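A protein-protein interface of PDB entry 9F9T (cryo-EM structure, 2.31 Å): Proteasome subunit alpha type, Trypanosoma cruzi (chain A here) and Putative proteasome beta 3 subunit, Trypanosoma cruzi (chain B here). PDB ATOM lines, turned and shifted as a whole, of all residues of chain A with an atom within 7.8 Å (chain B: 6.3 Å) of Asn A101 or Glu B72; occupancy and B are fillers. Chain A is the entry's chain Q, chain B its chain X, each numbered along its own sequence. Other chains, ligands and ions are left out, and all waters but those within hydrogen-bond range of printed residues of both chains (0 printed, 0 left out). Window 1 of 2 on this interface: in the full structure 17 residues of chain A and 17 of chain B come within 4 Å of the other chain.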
ATOM      1  N   ILE A  66     -17.281  -1.847  -5.796  1.00  0.00           N
ATOM      2  CA  ILE A  66     -16.832  -1.257  -4.547  1.00  0.00           C
ATOM      3  C   ILE A  66     -16.654  -2.374  -3.513  1.00  0.00           C
ATOM      4  O   ILE A  66     -15.895  -2.210  -2.556  1.00  0.00           O
ATOM      5  CB  ILE A  66     -17.813  -0.152  -4.066  1.00  0.00           C
ATOM      6  CG1 ILE A  66     -18.064   0.957  -5.095  1.00  0.00           C
ATOM      7  CG2 ILE A  66     -17.408   0.437  -2.726  1.00  0.00           C
ATOM      8  CD1 ILE A  66     -16.886   1.838  -5.363  1.00  0.00           C
ATOM      9  N   LYS A  73     -12.733  -1.989  -2.404  1.00  0.00           N
ATOM     10  CA  LYS A  73     -12.070  -0.743  -2.721  1.00  0.00           C
ATOM     11  C   LYS A  73     -11.707   0.002  -1.439  1.00  0.00           C
ATOM     12  O   LYS A  73     -12.461  -0.003  -0.455  1.00  0.00           O
ATOM     13  CB  LYS A  73     -13.030   0.072  -3.577  1.00  0.00           C
ATOM     14  CG  LYS A  73     -12.358   1.046  -4.531  1.00  0.00           C
ATOM     15  CD  LYS A  73     -13.383   1.974  -5.179  1.00  0.00           C
ATOM     16  CE  LYS A  73     -12.869   3.375  -5.416  1.00  0.00           C
ATOM     17  NZ  LYS A  73     -13.744   4.069  -6.410  1.00  0.00           N
ATOM     18  N   ILE A  74     -10.491   0.556  -1.412  1.00  0.00           N
ATOM     19  CA  ILE A  74     -10.112   1.503  -0.369  1.00  0.00           C
ATOM     20  C   ILE A  74     -10.063   2.925  -0.945  1.00  0.00           C
ATOM     21  O   ILE A  74     -10.360   3.872  -0.294  1.00  0.00           O
ATOM     22  CB  ILE A  74      -8.773   1.037   0.192  1.00  0.00           C
ATOM     23  CG1 ILE A  74      -8.952  -0.190   1.078  1.00  0.00           C
ATOM     24  CG2 ILE A  74      -8.058   2.140   0.958  1.00  0.00           C
ATOM     25  CD1 ILE A  74      -7.642  -0.700   1.601  1.00  0.00           C
ATOM     26  N   ALA A  75      -9.576   3.071  -2.149  1.00  0.00           N
ATOM     27  CA  ALA A  75      -9.558   4.283  -2.903  1.00  0.00           C
ATOM     28  C   ALA A  75      -9.307   3.897  -4.359  1.00  0.00           C
ATOM     29  O   ALA A  75      -9.159   2.742  -4.689  1.00  0.00           O
ATOM     30  CB  ALA A  75      -8.458   5.125  -2.347  1.00  0.00           C
ATOM     31  N   SER A  76      -9.276   4.831  -5.276  1.00  0.00           N
ATOM     32  CA  SER A  76      -9.360   4.439  -6.676  1.00  0.00           C
ATOM     33  C   SER A  76      -8.061   3.835  -7.188  1.00  0.00           C
ATOM     34  O   SER A  76      -8.019   3.416  -8.335  1.00  0.00           O
ATOM     35  CB  SER A  76      -9.701   5.634  -7.520  1.00  0.00           C
ATOM     36  OG  SER A  76      -8.517   6.222  -8.071  1.00  0.00           O
ATOM     37  N   HIS A  77      -6.980   3.914  -6.405  1.00  0.00           N
ATOM     38  CA  HIS A  77      -5.719   3.278  -6.757  1.00  0.00           C
ATOM     39  C   HIS A  77      -5.363   2.210  -5.722  1.00  0.00           C
ATOM     40  O   HIS A  77      -4.245   1.756  -5.706  1.00  0.00           O
ATOM     41  CB  HIS A  77      -4.580   4.321  -6.815  1.00  0.00           C
ATOM     42  CG  HIS A  77      -4.344   5.007  -5.509  1.00  0.00           C
ATOM     43  ND1 HIS A  77      -5.342   5.686  -4.813  1.00  0.00           N
ATOM     44  CD2 HIS A  77      -3.287   5.002  -4.676  1.00  0.00           C
ATOM     45  CE1 HIS A  77      -4.861   6.095  -3.636  1.00  0.00           C
ATOM     46  NE2 HIS A  77      -3.603   5.731  -3.546  1.00  0.00           N
ATOM     47  N   TYR A  95     -11.025   2.175   8.716  1.00  0.00           N
ATOM     48  CA  TYR A  95      -9.871   2.933   9.153  1.00  0.00           C
ATOM     49  C   TYR A  95      -9.044   3.360   7.945  1.00  0.00           C
ATOM     50  O   TYR A  95      -8.668   4.525   7.826  1.00  0.00           O
ATOM     51  CB  TYR A  95      -9.106   2.102  10.189  1.00  0.00           C
ATOM     52  CG  TYR A  95      -7.938   2.920  10.710  1.00  0.00           C
ATOM     53  CD1 TYR A  95      -8.148   3.983  11.588  1.00  0.00           C
ATOM     54  CD2 TYR A  95      -6.653   2.731  10.211  1.00  0.00           C
ATOM     55  CE1 TYR A  95      -7.102   4.798  11.988  1.00  0.00           C
ATOM     56  CE2 TYR A  95      -5.606   3.551  10.591  1.00  0.00           C
ATOM     57  CZ  TYR A  95      -5.825   4.580  11.487  1.00  0.00           C
ATOM     58  OH  TYR A  95      -4.765   5.364  11.860  1.00  0.00           O
ATOM     59  N   ALA A  96      -8.834   2.417   7.027  1.00  0.00           N
ATOM     60  CA  ALA A  96      -8.029   2.656   5.852  1.00  0.00           C
ATOM     61  C   ALA A  96      -8.693   3.596   4.842  1.00  0.00           C
ATOM     62  O   ALA A  96      -8.016   4.451   4.252  1.00  0.00           O
ATOM     63  CB  ALA A  96      -7.720   1.350   5.205  1.00  0.00           C
ATOM     64  N   ARG A  97     -10.015   3.455   4.644  1.00  0.00           N
ATOM     65  CA  ARG A  97     -10.730   4.358   3.750  1.00  0.00           C
ATOM     66  C   ARG A  97     -10.614   5.805   4.247  1.00  0.00           C
ATOM     67  O   ARG A  97     -10.398   6.735   3.482  1.00  0.00           O
ATOM     68  CB  ARG A  97     -12.178   3.908   3.605  1.00  0.00           C
ATOM     69  CG  ARG A  97     -12.312   2.784   2.596  1.00  0.00           C
ATOM     70  CD  ARG A  97     -13.688   2.219   2.686  1.00  0.00           C
ATOM     71  NE  ARG A  97     -13.828   1.259   1.620  1.00  0.00           N
ATOM     72  CZ  ARG A  97     -14.890   0.493   1.503  1.00  0.00           C
ATOM     73  NH1 ARG A  97     -15.029  -0.306   0.472  1.00  0.00           N
ATOM     74  NH2 ARG A  97     -15.830   0.553   2.429  1.00  0.00           N
ATOM     75  N   LEU A  98     -10.767   5.970   5.536  1.00  0.00           N
ATOM     76  CA  LEU A  98     -10.708   7.274   6.159  1.00  0.00           C
ATOM     77  C   LEU A  98      -9.294   7.844   6.105  1.00  0.00           C
ATOM     78  O   LEU A  98      -9.119   8.994   5.728  1.00  0.00           O
ATOM     79  CB  LEU A  98     -11.211   6.981   7.562  1.00  0.00           C
ATOM     80  CG  LEU A  98     -11.676   8.128   8.415  1.00  0.00           C
ATOM     81  CD1 LEU A  98     -12.380   7.603   9.666  1.00  0.00           C
ATOM     82  CD2 LEU A  98     -10.479   8.953   8.795  1.00  0.00           C
ATOM     83  N   SER A  99      -8.251   7.024   6.252  1.00  0.00           N
ATOM     84  CA  SER A  99      -6.891   7.536   6.189  1.00  0.00           C
ATOM     85  C   SER A  99      -6.501   7.918   4.795  1.00  0.00           C
ATOM     86  O   SER A  99      -5.655   8.792   4.654  1.00  0.00           O
ATOM     87  CB  SER A  99      -5.855   6.589   6.678  1.00  0.00           C
ATOM     88  OG  SER A  99      -6.377   5.874   7.805  1.00  0.00           O
ATOM     89  N   ALA A 100      -6.976   7.155   3.808  1.00  0.00           N
ATOM     90  CA  ALA A 100      -6.616   7.424   2.419  1.00  0.00           C
ATOM     91  C   ALA A 100      -7.226   8.733   1.976  1.00  0.00           C
ATOM     92  O   ALA A 100      -6.599   9.504   1.265  1.00  0.00           O
ATOM     93  CB  ALA A 100      -7.101   6.312   1.522  1.00  0.00           C
ATOM     94  N   ASN A 101      -8.431   9.004   2.460  1.00  0.00           N
ATOM     95  CA  ASN A 101      -9.162  10.210   2.090  1.00  0.00           C
ATOM     96  C   ASN A 101      -8.702  11.434   2.849  1.00  0.00           C
ATOM     97  O   ASN A 101      -8.687  12.493   2.246  1.00  0.00           O
ATOM     98  CB  ASN A 101     -10.669  10.013   2.171  1.00  0.00           C
ATOM     99  CG  ASN A 101     -11.121   9.602   0.797  1.00  0.00           C
ATOM    100  OD1 ASN A 101     -11.404  10.470  -0.022  1.00  0.00           O
ATOM    101  ND2 ASN A 101     -10.959   8.318   0.483  1.00  0.00           N
ATOM    102  N   ARG A 102      -8.292  11.277   4.119  1.00  0.00           N
ATOM    103  CA  ARG A 102      -7.576  12.354   4.793  1.00  0.00           C
ATOM    104  C   ARG A 102      -6.349  12.789   4.003  1.00  0.00           C
ATOM    105  O   ARG A 102      -6.002  13.968   4.035  1.00  0.00           O
ATOM    106  CB  ARG A 102      -7.067  11.973   6.174  1.00  0.00           C
ATOM    107  CG  ARG A 102      -8.143  11.962   7.248  1.00  0.00           C
ATOM    108  CD  ARG A 102      -7.515  11.619   8.601  1.00  0.00           C
ATOM    109  NE  ARG A 102      -8.385  11.015   9.611  1.00  0.00           N
ATOM    110  CZ  ARG A 102      -9.507  11.568  10.099  1.00  0.00           C
ATOM    111  NH1 ARG A 102     -10.070  11.055  11.185  1.00  0.00           N
ATOM    112  NH2 ARG A 102     -10.056  12.636   9.529  1.00  0.00           N
ATOM    113  N   HIS A 103      -5.611  11.839   3.383  1.00  0.00           N
ATOM    114  CA  HIS A 103      -4.374  12.215   2.736  1.00  0.00           C
ATOM    115  C   HIS A 103      -4.708  13.015   1.479  1.00  0.00           C
ATOM    116  O   HIS A 103      -4.119  14.039   1.179  1.00  0.00           O
ATOM    117  CB  HIS A 103      -3.581  10.953   2.446  1.00  0.00           C
ATOM    118  CG  HIS A 103      -2.265  11.155   1.816  1.00  0.00           C
ATOM    119  ND1 HIS A 103      -2.145  11.473   0.473  1.00  0.00           N
ATOM    120  CD2 HIS A 103      -1.006  11.133   2.356  1.00  0.00           C
ATOM    121  CE1 HIS A 103      -0.827  11.610   0.223  1.00  0.00           C
ATOM    122  NE2 HIS A 103      -0.133  11.414   1.378  1.00  0.00           N
ATOM    123  N   HIS A 104      -5.708  12.565   0.738  1.00  0.00           N
ATOM    124  CA  HIS A 104      -6.208  13.362  -0.357  1.00  0.00           C
ATOM    125  C   HIS A 104      -6.664  14.755   0.132  1.00  0.00           C
ATOM    126  O   HIS A 104      -6.356  15.780  -0.464  1.00  0.00           O
ATOM    127  CB  HIS A 104      -7.277  12.583  -1.103  1.00  0.00           C
ATOM    128  CG  HIS A 104      -7.398  13.120  -2.456  1.00  0.00           C
ATOM    129  ND1 HIS A 104      -8.079  14.289  -2.733  1.00  0.00           N
ATOM    130  CD2 HIS A 104      -6.872  12.684  -3.590  1.00  0.00           C
ATOM    131  CE1 HIS A 104      -7.933  14.575  -4.050  1.00  0.00           C
ATOM    132  NE2 HIS A 104      -7.215  13.591  -4.606  1.00  0.00           N
ATOM    133  N   TYR A 105      -7.295  14.802   1.298  1.00  0.00           N
ATOM    134  CA  TYR A 105      -7.735  16.076   1.774  1.00  0.00           C
ATOM    135  C   TYR A 105      -6.561  17.008   1.975  1.00  0.00           C
ATOM    136  O   TYR A 105      -6.614  18.173   1.615  1.00  0.00           O
ATOM    137  CB  TYR A 105      -8.561  15.963   3.039  1.00  0.00           C
ATOM    138  CG  TYR A 105      -8.983  17.322   3.554  1.00  0.00           C
ATOM    139  CD1 TYR A 105     -10.071  17.984   3.015  1.00  0.00           C
ATOM    140  CD2 TYR A 105      -8.279  17.947   4.572  1.00  0.00           C
ATOM    141  CE1 TYR A 105     -10.492  19.203   3.519  1.00  0.00           C
ATOM    142  CE2 TYR A 105      -8.674  19.173   5.074  1.00  0.00           C
ATOM    143  CZ  TYR A 105      -9.784  19.807   4.543  1.00  0.00           C
ATOM    144  OH  TYR A 105     -10.152  21.045   4.994  1.00  0.00           O
ATOM    145  N   THR A 106      -5.498  16.511   2.556  1.00  0.00           N
ATOM    146  CA  THR A 106      -4.393  17.350   2.905  1.00  0.00           C
ATOM    147  C   THR A 106      -3.491  17.660   1.707  1.00  0.00           C
ATOM    148  O   THR A 106      -3.192  18.804   1.494  1.00  0.00           O
ATOM    149  CB  THR A 106      -3.557  16.686   3.973  1.00  0.00           C
ATOM    150  OG1 THR A 106      -4.380  16.367   5.083  1.00  0.00           O
ATOM    151  CG2 THR A 106      -2.456  17.621   4.402  1.00  0.00           C
ATOM    152  N   TYR A 107      -3.045  16.678   0.938  1.00  0.00           N
ATOM    153  CA  TYR A 107      -2.072  16.918  -0.119  1.00  0.00           C
ATOM    154  C   TYR A 107      -2.661  16.981  -1.510  1.00  0.00           C
ATOM    155  O   TYR A 107      -1.912  17.135  -2.458  1.00  0.00           O
ATOM    156  CB  TYR A 107      -1.147  15.708  -0.101  1.00  0.00           C
ATOM    157  CG  TYR A 107      -0.369  15.676   1.196  1.00  0.00           C
ATOM    158  CD1 TYR A 107       0.686  16.531   1.401  1.00  0.00           C
ATOM    159  CD2 TYR A 107      -0.719  14.832   2.217  1.00  0.00           C
ATOM    160  CE1 TYR A 107       1.375  16.529   2.601  1.00  0.00           C
ATOM    161  CE2 TYR A 107      -0.056  14.823   3.421  1.00  0.00           C
ATOM    162  CZ  TYR A 107       1.021  15.656   3.610  1.00  0.00           C
ATOM    163  OH  TYR A 107       1.713  15.659   4.801  1.00  0.00           O
ATOM    164  N   GLN A 108      -3.994  16.806  -1.628  1.00  0.00           N
ATOM    165  CA  GLN A 108      -4.678  16.676  -2.911  1.00  0.00           C
ATOM    166  C   GLN A 108      -3.931  15.783  -3.896  1.00  0.00           C
ATOM    167  O   GLN A 108      -3.885  16.079  -5.076  1.00  0.00           O
ATOM    168  CB  GLN A 108      -4.886  18.027  -3.602  1.00  0.00           C
ATOM    169  CG  GLN A 108      -5.756  18.976  -2.801  1.00  0.00           C
ATOM    170  CD  GLN A 108      -7.183  18.512  -2.613  1.00  0.00           C
ATOM    171  OE1 GLN A 108      -7.829  18.051  -3.559  1.00  0.00           O
ATOM    172  NE2 GLN A 108      -7.679  18.616  -1.384  1.00  0.00           N
ATOM    173  N   GLU A 109      -3.460  14.643  -3.425  1.00  0.00           N
ATOM    174  CA  GLU A 109      -2.787  13.679  -4.267  1.00  0.00           C
ATOM    175  C   GLU A 109      -3.067  12.304  -3.647  1.00  0.00           C
ATOM    176  O   GLU A 109      -3.352  12.179  -2.479  1.00  0.00           O
ATOM    177  CB  GLU A 109      -1.284  14.013  -4.378  1.00  0.00           C
ATOM    178  CG  GLU A 109      -0.479  13.335  -3.253  1.00  0.00           C
ATOM    179  CD  GLU A 109       1.048  13.434  -3.141  1.00  0.00           C
ATOM    180  OE1 GLU A 109       1.549  13.269  -1.964  1.00  0.00           O
ATOM    181  OE2 GLU A 109       1.759  13.645  -4.199  1.00  0.00           O
ATOM    182  N   MET A 111      -2.686   8.733  -1.834  1.00  0.00           N
ATOM    183  CA  MET A 111      -1.711   8.245  -0.877  1.00  0.00           C
ATOM    184  C   MET A 111      -0.920   7.112  -1.520  1.00  0.00           C
ATOM    185  O   MET A 111      -1.469   6.346  -2.304  1.00  0.00           O
ATOM    186  CB  MET A 111      -2.464   7.751   0.351  1.00  0.00           C
ATOM    187  CG  MET A 111      -1.617   7.184   1.470  1.00  0.00           C
ATOM    188  SD  MET A 111      -2.694   6.969   2.909  1.00  0.00           S
ATOM    189  CE  MET A 111      -1.584   7.483   4.202  1.00  0.00           C
ATOM    190  N   LEU A 116      -0.013   3.763   3.023  1.00  0.00           N
ATOM    191  CA  LEU A 116      -1.336   3.352   3.491  1.00  0.00           C
ATOM    192  C   LEU A 116      -1.203   2.111   4.355  1.00  0.00           C
ATOM    193  O   LEU A 116      -1.800   1.999   5.409  1.00  0.00           O
ATOM    194  CB  LEU A 116      -2.311   3.070   2.329  1.00  0.00           C
ATOM    195  CG  LEU A 116      -3.749   2.672   2.728  1.00  0.00           C
ATOM    196  CD1 LEU A 116      -3.872   1.180   2.952  1.00  0.00           C
ATOM    197  CD2 LEU A 116      -4.244   3.388   3.985  1.00  0.00           C
ATOM    198  N   VAL B  67     -16.506  18.997   1.212  1.00  0.00           N
ATOM    199  CA  VAL B  67     -17.577  18.395   0.444  1.00  0.00           C
ATOM    200  C   VAL B  67     -17.036  17.218  -0.323  1.00  0.00           C
ATOM    201  O   VAL B  67     -17.676  16.205  -0.305  1.00  0.00           O
ATOM    202  CB  VAL B  67     -18.225  19.459  -0.495  1.00  0.00           C
ATOM    203  CG1 VAL B  67     -19.219  18.909  -1.480  1.00  0.00           C
ATOM    204  CG2 VAL B  67     -18.969  20.498   0.278  1.00  0.00           C
ATOM    205  N   ARG B  68     -15.888  17.376  -0.988  1.00  0.00           N
ATOM    206  CA  ARG B  68     -15.261  16.304  -1.745  1.00  0.00           C
ATOM    207  C   ARG B  68     -14.898  15.155  -0.817  1.00  0.00           C
ATOM    208  O   ARG B  68     -15.267  14.026  -1.078  1.00  0.00           O
ATOM    209  CB  ARG B  68     -14.083  16.764  -2.591  1.00  0.00           C
ATOM    210  CG  ARG B  68     -14.512  17.570  -3.808  1.00  0.00           C
ATOM    211  CD  ARG B  68     -13.589  17.552  -5.028  1.00  0.00           C
ATOM    212  NE  ARG B  68     -12.624  18.657  -4.961  1.00  0.00           N
ATOM    213  CZ  ARG B  68     -11.320  18.536  -4.698  1.00  0.00           C
ATOM    214  NH1 ARG B  68     -10.626  19.590  -4.297  1.00  0.00           N
ATOM    215  NH2 ARG B  68     -10.743  17.345  -4.727  1.00  0.00           N
ATOM    216  N   PHE B  69     -14.281  15.421   0.306  1.00  0.00           N
ATOM    217  CA  PHE B  69     -13.953  14.379   1.246  1.00  0.00           C
ATOM    218  C   PHE B  69     -15.197  13.596   1.658  1.00  0.00           C
ATOM    219  O   PHE B  69     -15.214  12.389   1.531  1.00  0.00           O
ATOM    220  CB  PHE B  69     -13.187  15.009   2.406  1.00  0.00           C
ATOM    221  CG  PHE B  69     -12.912  14.127   3.597  1.00  0.00           C
ATOM    222  CD1 PHE B  69     -13.798  14.073   4.658  1.00  0.00           C
ATOM    223  CD2 PHE B  69     -11.719  13.443   3.705  1.00  0.00           C
ATOM    224  CE1 PHE B  69     -13.537  13.290   5.775  1.00  0.00           C
ATOM    225  CE2 PHE B  69     -11.442  12.692   4.829  1.00  0.00           C
ATOM    226  CZ  PHE B  69     -12.348  12.622   5.867  1.00  0.00           C
ATOM    227  N   ARG B  70     -16.270  14.251   2.101  1.00  0.00           N
ATOM    228  CA  ARG B  70     -17.462  13.536   2.552  1.00  0.00           C
ATOM    229  C   ARG B  70     -18.143  12.759   1.435  1.00  0.00           C
ATOM    230  O   ARG B  70     -18.824  11.805   1.639  1.00  0.00           O
ATOM    231  CB  ARG B  70     -18.519  14.496   3.094  1.00  0.00           C
ATOM    232  CG  ARG B  70     -18.022  15.316   4.263  1.00  0.00           C
ATOM    233  CD  ARG B  70     -18.178  14.604   5.557  1.00  0.00           C
ATOM    234  NE  ARG B  70     -19.570  14.793   5.969  1.00  0.00           N
ATOM    235  CZ  ARG B  70     -19.964  15.708   6.851  1.00  0.00           C
ATOM    236  NH1 ARG B  70     -19.194  16.753   7.125  1.00  0.00           N
ATOM    237  NH2 ARG B  70     -21.125  15.560   7.457  1.00  0.00           N
ATOM    238  N   ASN B  71     -18.017  13.234   0.237  1.00  0.00           N
ATOM    239  CA  ASN B  71     -18.662  12.584  -0.867  1.00  0.00           C
ATOM    240  C   ASN B  71     -17.970  11.271  -1.195  1.00  0.00           C
ATOM    241  O   ASN B  71     -18.642  10.298  -1.428  1.00  0.00           O
ATOM    242  CB  ASN B  71     -18.555  13.448  -2.126  1.00  0.00           C
ATOM    243  CG  ASN B  71     -19.478  12.953  -3.217  1.00  0.00           C
ATOM    244  OD1 ASN B  71     -20.485  12.298  -2.947  1.00  0.00           O
ATOM    245  ND2 ASN B  71     -19.180  13.308  -4.443  1.00  0.00           N
ATOM    246  N   GLU B  72     -16.623  11.290  -1.284  1.00  0.00           N
ATOM    247  CA  GLU B  72     -15.825  10.087  -1.406  1.00  0.00           C
ATOM    248  C   GLU B  72     -16.148   9.043  -0.350  1.00  0.00           C
ATOM    249  O   GLU B  72     -16.414   7.901  -0.685  1.00  0.00           O
ATOM    250  CB  GLU B  72     -14.358  10.399  -1.263  1.00  0.00           C
ATOM    251  CG  GLU B  72     -13.834  11.275  -2.409  1.00  0.00           C
ATOM    252  CD  GLU B  72     -14.173  10.838  -3.836  1.00  0.00           C
ATOM    253  OE1 GLU B  72     -14.476  11.736  -4.680  1.00  0.00           O
ATOM    254  OE2 GLU B  72     -14.107   9.601  -4.113  1.00  0.00           O
ATOM    255  N   LEU B  73     -16.238   9.420   0.917  1.00  0.00           N
ATOM    256  CA  LEU B  73     -16.597   8.424   1.908  1.00  0.00           C
ATOM    257  C   LEU B  73     -18.005   7.944   1.713  1.00  0.00           C
ATOM    258  O   LEU B  73     -18.298   6.815   2.035  1.00  0.00           O
ATOM    259  CB  LEU B  73     -16.461   8.984   3.308  1.00  0.00           C
ATOM    260  CG  LEU B  73     -15.032   9.123   3.848  1.00  0.00           C
ATOM    261  CD1 LEU B  73     -15.143   9.417   5.314  1.00  0.00           C
ATOM    262  CD2 LEU B  73     -14.170   7.885   3.663  1.00  0.00           C
ATOM    263  N   TYR B  74     -18.917   8.797   1.237  1.00  0.00           N
ATOM    264  CA  TYR B  74     -20.318   8.403   1.046  1.00  0.00           C
ATOM    265  C   TYR B  74     -20.388   7.296   0.002  1.00  0.00           C
ATOM    266  O   TYR B  74     -21.073   6.308   0.205  1.00  0.00           O
ATOM    267  CB  TYR B  74     -21.083   9.659   0.535  1.00  0.00           C
ATOM    268  CG  TYR B  74     -22.542   9.445   0.153  1.00  0.00           C
ATOM    269  CD1 TYR B  74     -22.945   8.897  -1.044  1.00  0.00           C
ATOM    270  CD2 TYR B  74     -23.517   9.737   1.074  1.00  0.00           C
ATOM    271  CE1 TYR B  74     -24.273   8.630  -1.308  1.00  0.00           C
ATOM    272  CE2 TYR B  74     -24.867   9.608   0.795  1.00  0.00           C
ATOM    273  CZ  TYR B  74     -25.247   9.029  -0.389  1.00  0.00           C
ATOM    274  OH  TYR B  74     -26.594   8.965  -0.451  1.00  0.00           O
ATOM    275  N   LYS B  75     -19.700   7.541  -1.121  1.00  0.00           N
ATOM    276  CA  LYS B  75     -19.646   6.622  -2.244  1.00  0.00           C
ATOM    277  C   LYS B  75     -19.080   5.255  -1.898  1.00  0.00           C
ATOM    278  O   LYS B  75     -19.480   4.293  -2.546  1.00  0.00           O
ATOM    279  CB  LYS B  75     -18.772   7.136  -3.377  1.00  0.00           C
ATOM    280  CG  LYS B  75     -19.414   8.290  -4.145  1.00  0.00           C
ATOM    281  CD  LYS B  75     -18.700   8.657  -5.389  1.00  0.00           C
ATOM    282  CE  LYS B  75     -17.615   9.662  -5.097  1.00  0.00           C
ATOM    283  NZ  LYS B  75     -16.713   9.800  -6.268  1.00  0.00           N
ATOM    284  N   LEU B  76     -18.198   5.139  -0.896  1.00  0.00           N
ATOM    285  CA  LEU B  76     -17.631   3.847  -0.526  1.00  0.00           C
ATOM    286  C   LEU B  76     -18.553   3.123   0.446  1.00  0.00           C
ATOM    287  O   LEU B  76     -18.798   1.959   0.264  1.00  0.00           O
ATOM    288  CB  LEU B  76     -16.268   4.079   0.127  1.00  0.00           C
ATOM    289  CG  LEU B  76     -15.175   4.530  -0.817  1.00  0.00           C
ATOM    290  CD1 LEU B  76     -13.939   5.016  -0.081  1.00  0.00           C
ATOM    291  CD2 LEU B  76     -14.809   3.397  -1.726  1.00  0.00           C
ATOM    292  N   ARG B  77     -18.993   3.778   1.527  1.00  0.00           N
ATOM    293  CA  ARG B  77     -20.046   3.238   2.363  1.00  0.00           C
ATOM    294  C   ARG B  77     -21.298   2.826   1.593  1.00  0.00           C
ATOM    295  O   ARG B  77     -21.880   1.814   1.861  1.00  0.00           O
ATOM    296  CB  ARG B  77     -20.617   4.283   3.327  1.00  0.00           C
ATOM    297  CG  ARG B  77     -19.655   4.792   4.386  1.00  0.00           C
ATOM    298  CD  ARG B  77     -20.394   5.581   5.486  1.00  0.00           C
ATOM    299  NE  ARG B  77     -21.103   6.792   5.056  1.00  0.00           N
ATOM    300  CZ  ARG B  77     -20.612   8.035   4.916  1.00  0.00           C
ATOM    301  NH1 ARG B  77     -19.449   8.377   5.410  1.00  0.00           N
ATOM    302  NH2 ARG B  77     -21.320   8.967   4.303  1.00  0.00           N
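Ala A75 touches none of the printed residues of chain B. Of the printed residues of chain B, Arg A97 touches Leu B73 (3.9 Å) and Leu B76 (3.8 Å). Of chain B, only Phe B69 and Glu B72 come within 4 Å of Asn A101. Glu B72 touches one residue of chain A. Of the printed residues of chain A, Leu B73 touches Arg A97 (3.9 Å). The nearest residue of chain B that does not touch Asn A101 is Leu B73 (4.4 Å). The nearest residue of chain A that does not touch Glu B72 is Lys A73 (6.0 Å). The nearest printed residue of chain A that does not touch Arg B68 is His A104 (4.003 Å).
The guanidinium group of Arg B68 sits at hydrogen-bond distance from the side-chain amide oxygen of Gln A108.
Printed residues of chain B that touch a printed residue of chain A: Arg B68, Phe B69, Glu B72, Leu B73 and Leu B76. Hydrophobic or aromatic side chains of chain B within 4 Å of the printed part of chain A: Phe B69, Leu B73 and Leu B76. Hydrophobic or aromatic side chains of chain A within 4 Å of the printed part of chain B: Ile A66. Among the printed residues, 9 pairs touch across the chains. Among the printed residues, no Asp or Glu carboxylate lies within 4 Å of a Lys or Arg side-chain nitrogen of the other chain.
CG2 of Ile A66 touches O of Leu B76 (3.6 Å). Lys A73 touches Leu B76. Leu B76 touches Ile A74 (CD1 to O, 3.8 Å). Leu B73 touches Arg A97 (CD2 to O, 3.9 Å). Leu B76 touches Arg A97 (CD1 to CG, 3.8 Å). Phe B69 touches Asn A101 (CD2 to O, 3.5 Å). Glu B72 touches Asn A101. Arg A102 touches Phe B69.
The side-chain carboxylate (OE1) of Glu B72 lies within salt-bridge range of the side-chain amino group (NZ) of Lys B75, 3.4 Å away. N of Lys A73 lies within hydrogen-bond range of O of Ile A66 (3.2 Å). ND2 of Asn A101 lies within hydrogen-bond range of O of Arg A97 (3.4 Å). OG1 of Thr A106 is in hydrogen-bond range of O of Arg A102, 3.1 Å away. The side-chain amide nitrogen of Gln A108 sits close to the backbone carbonyl oxygen of His A104 (3.3 Å). The backbone carbonyl oxygen (O) of Tyr A105 is in hydrogen-bond range of the side-chain amide nitrogen (NE2) of Gln A108 (3.2 Å).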
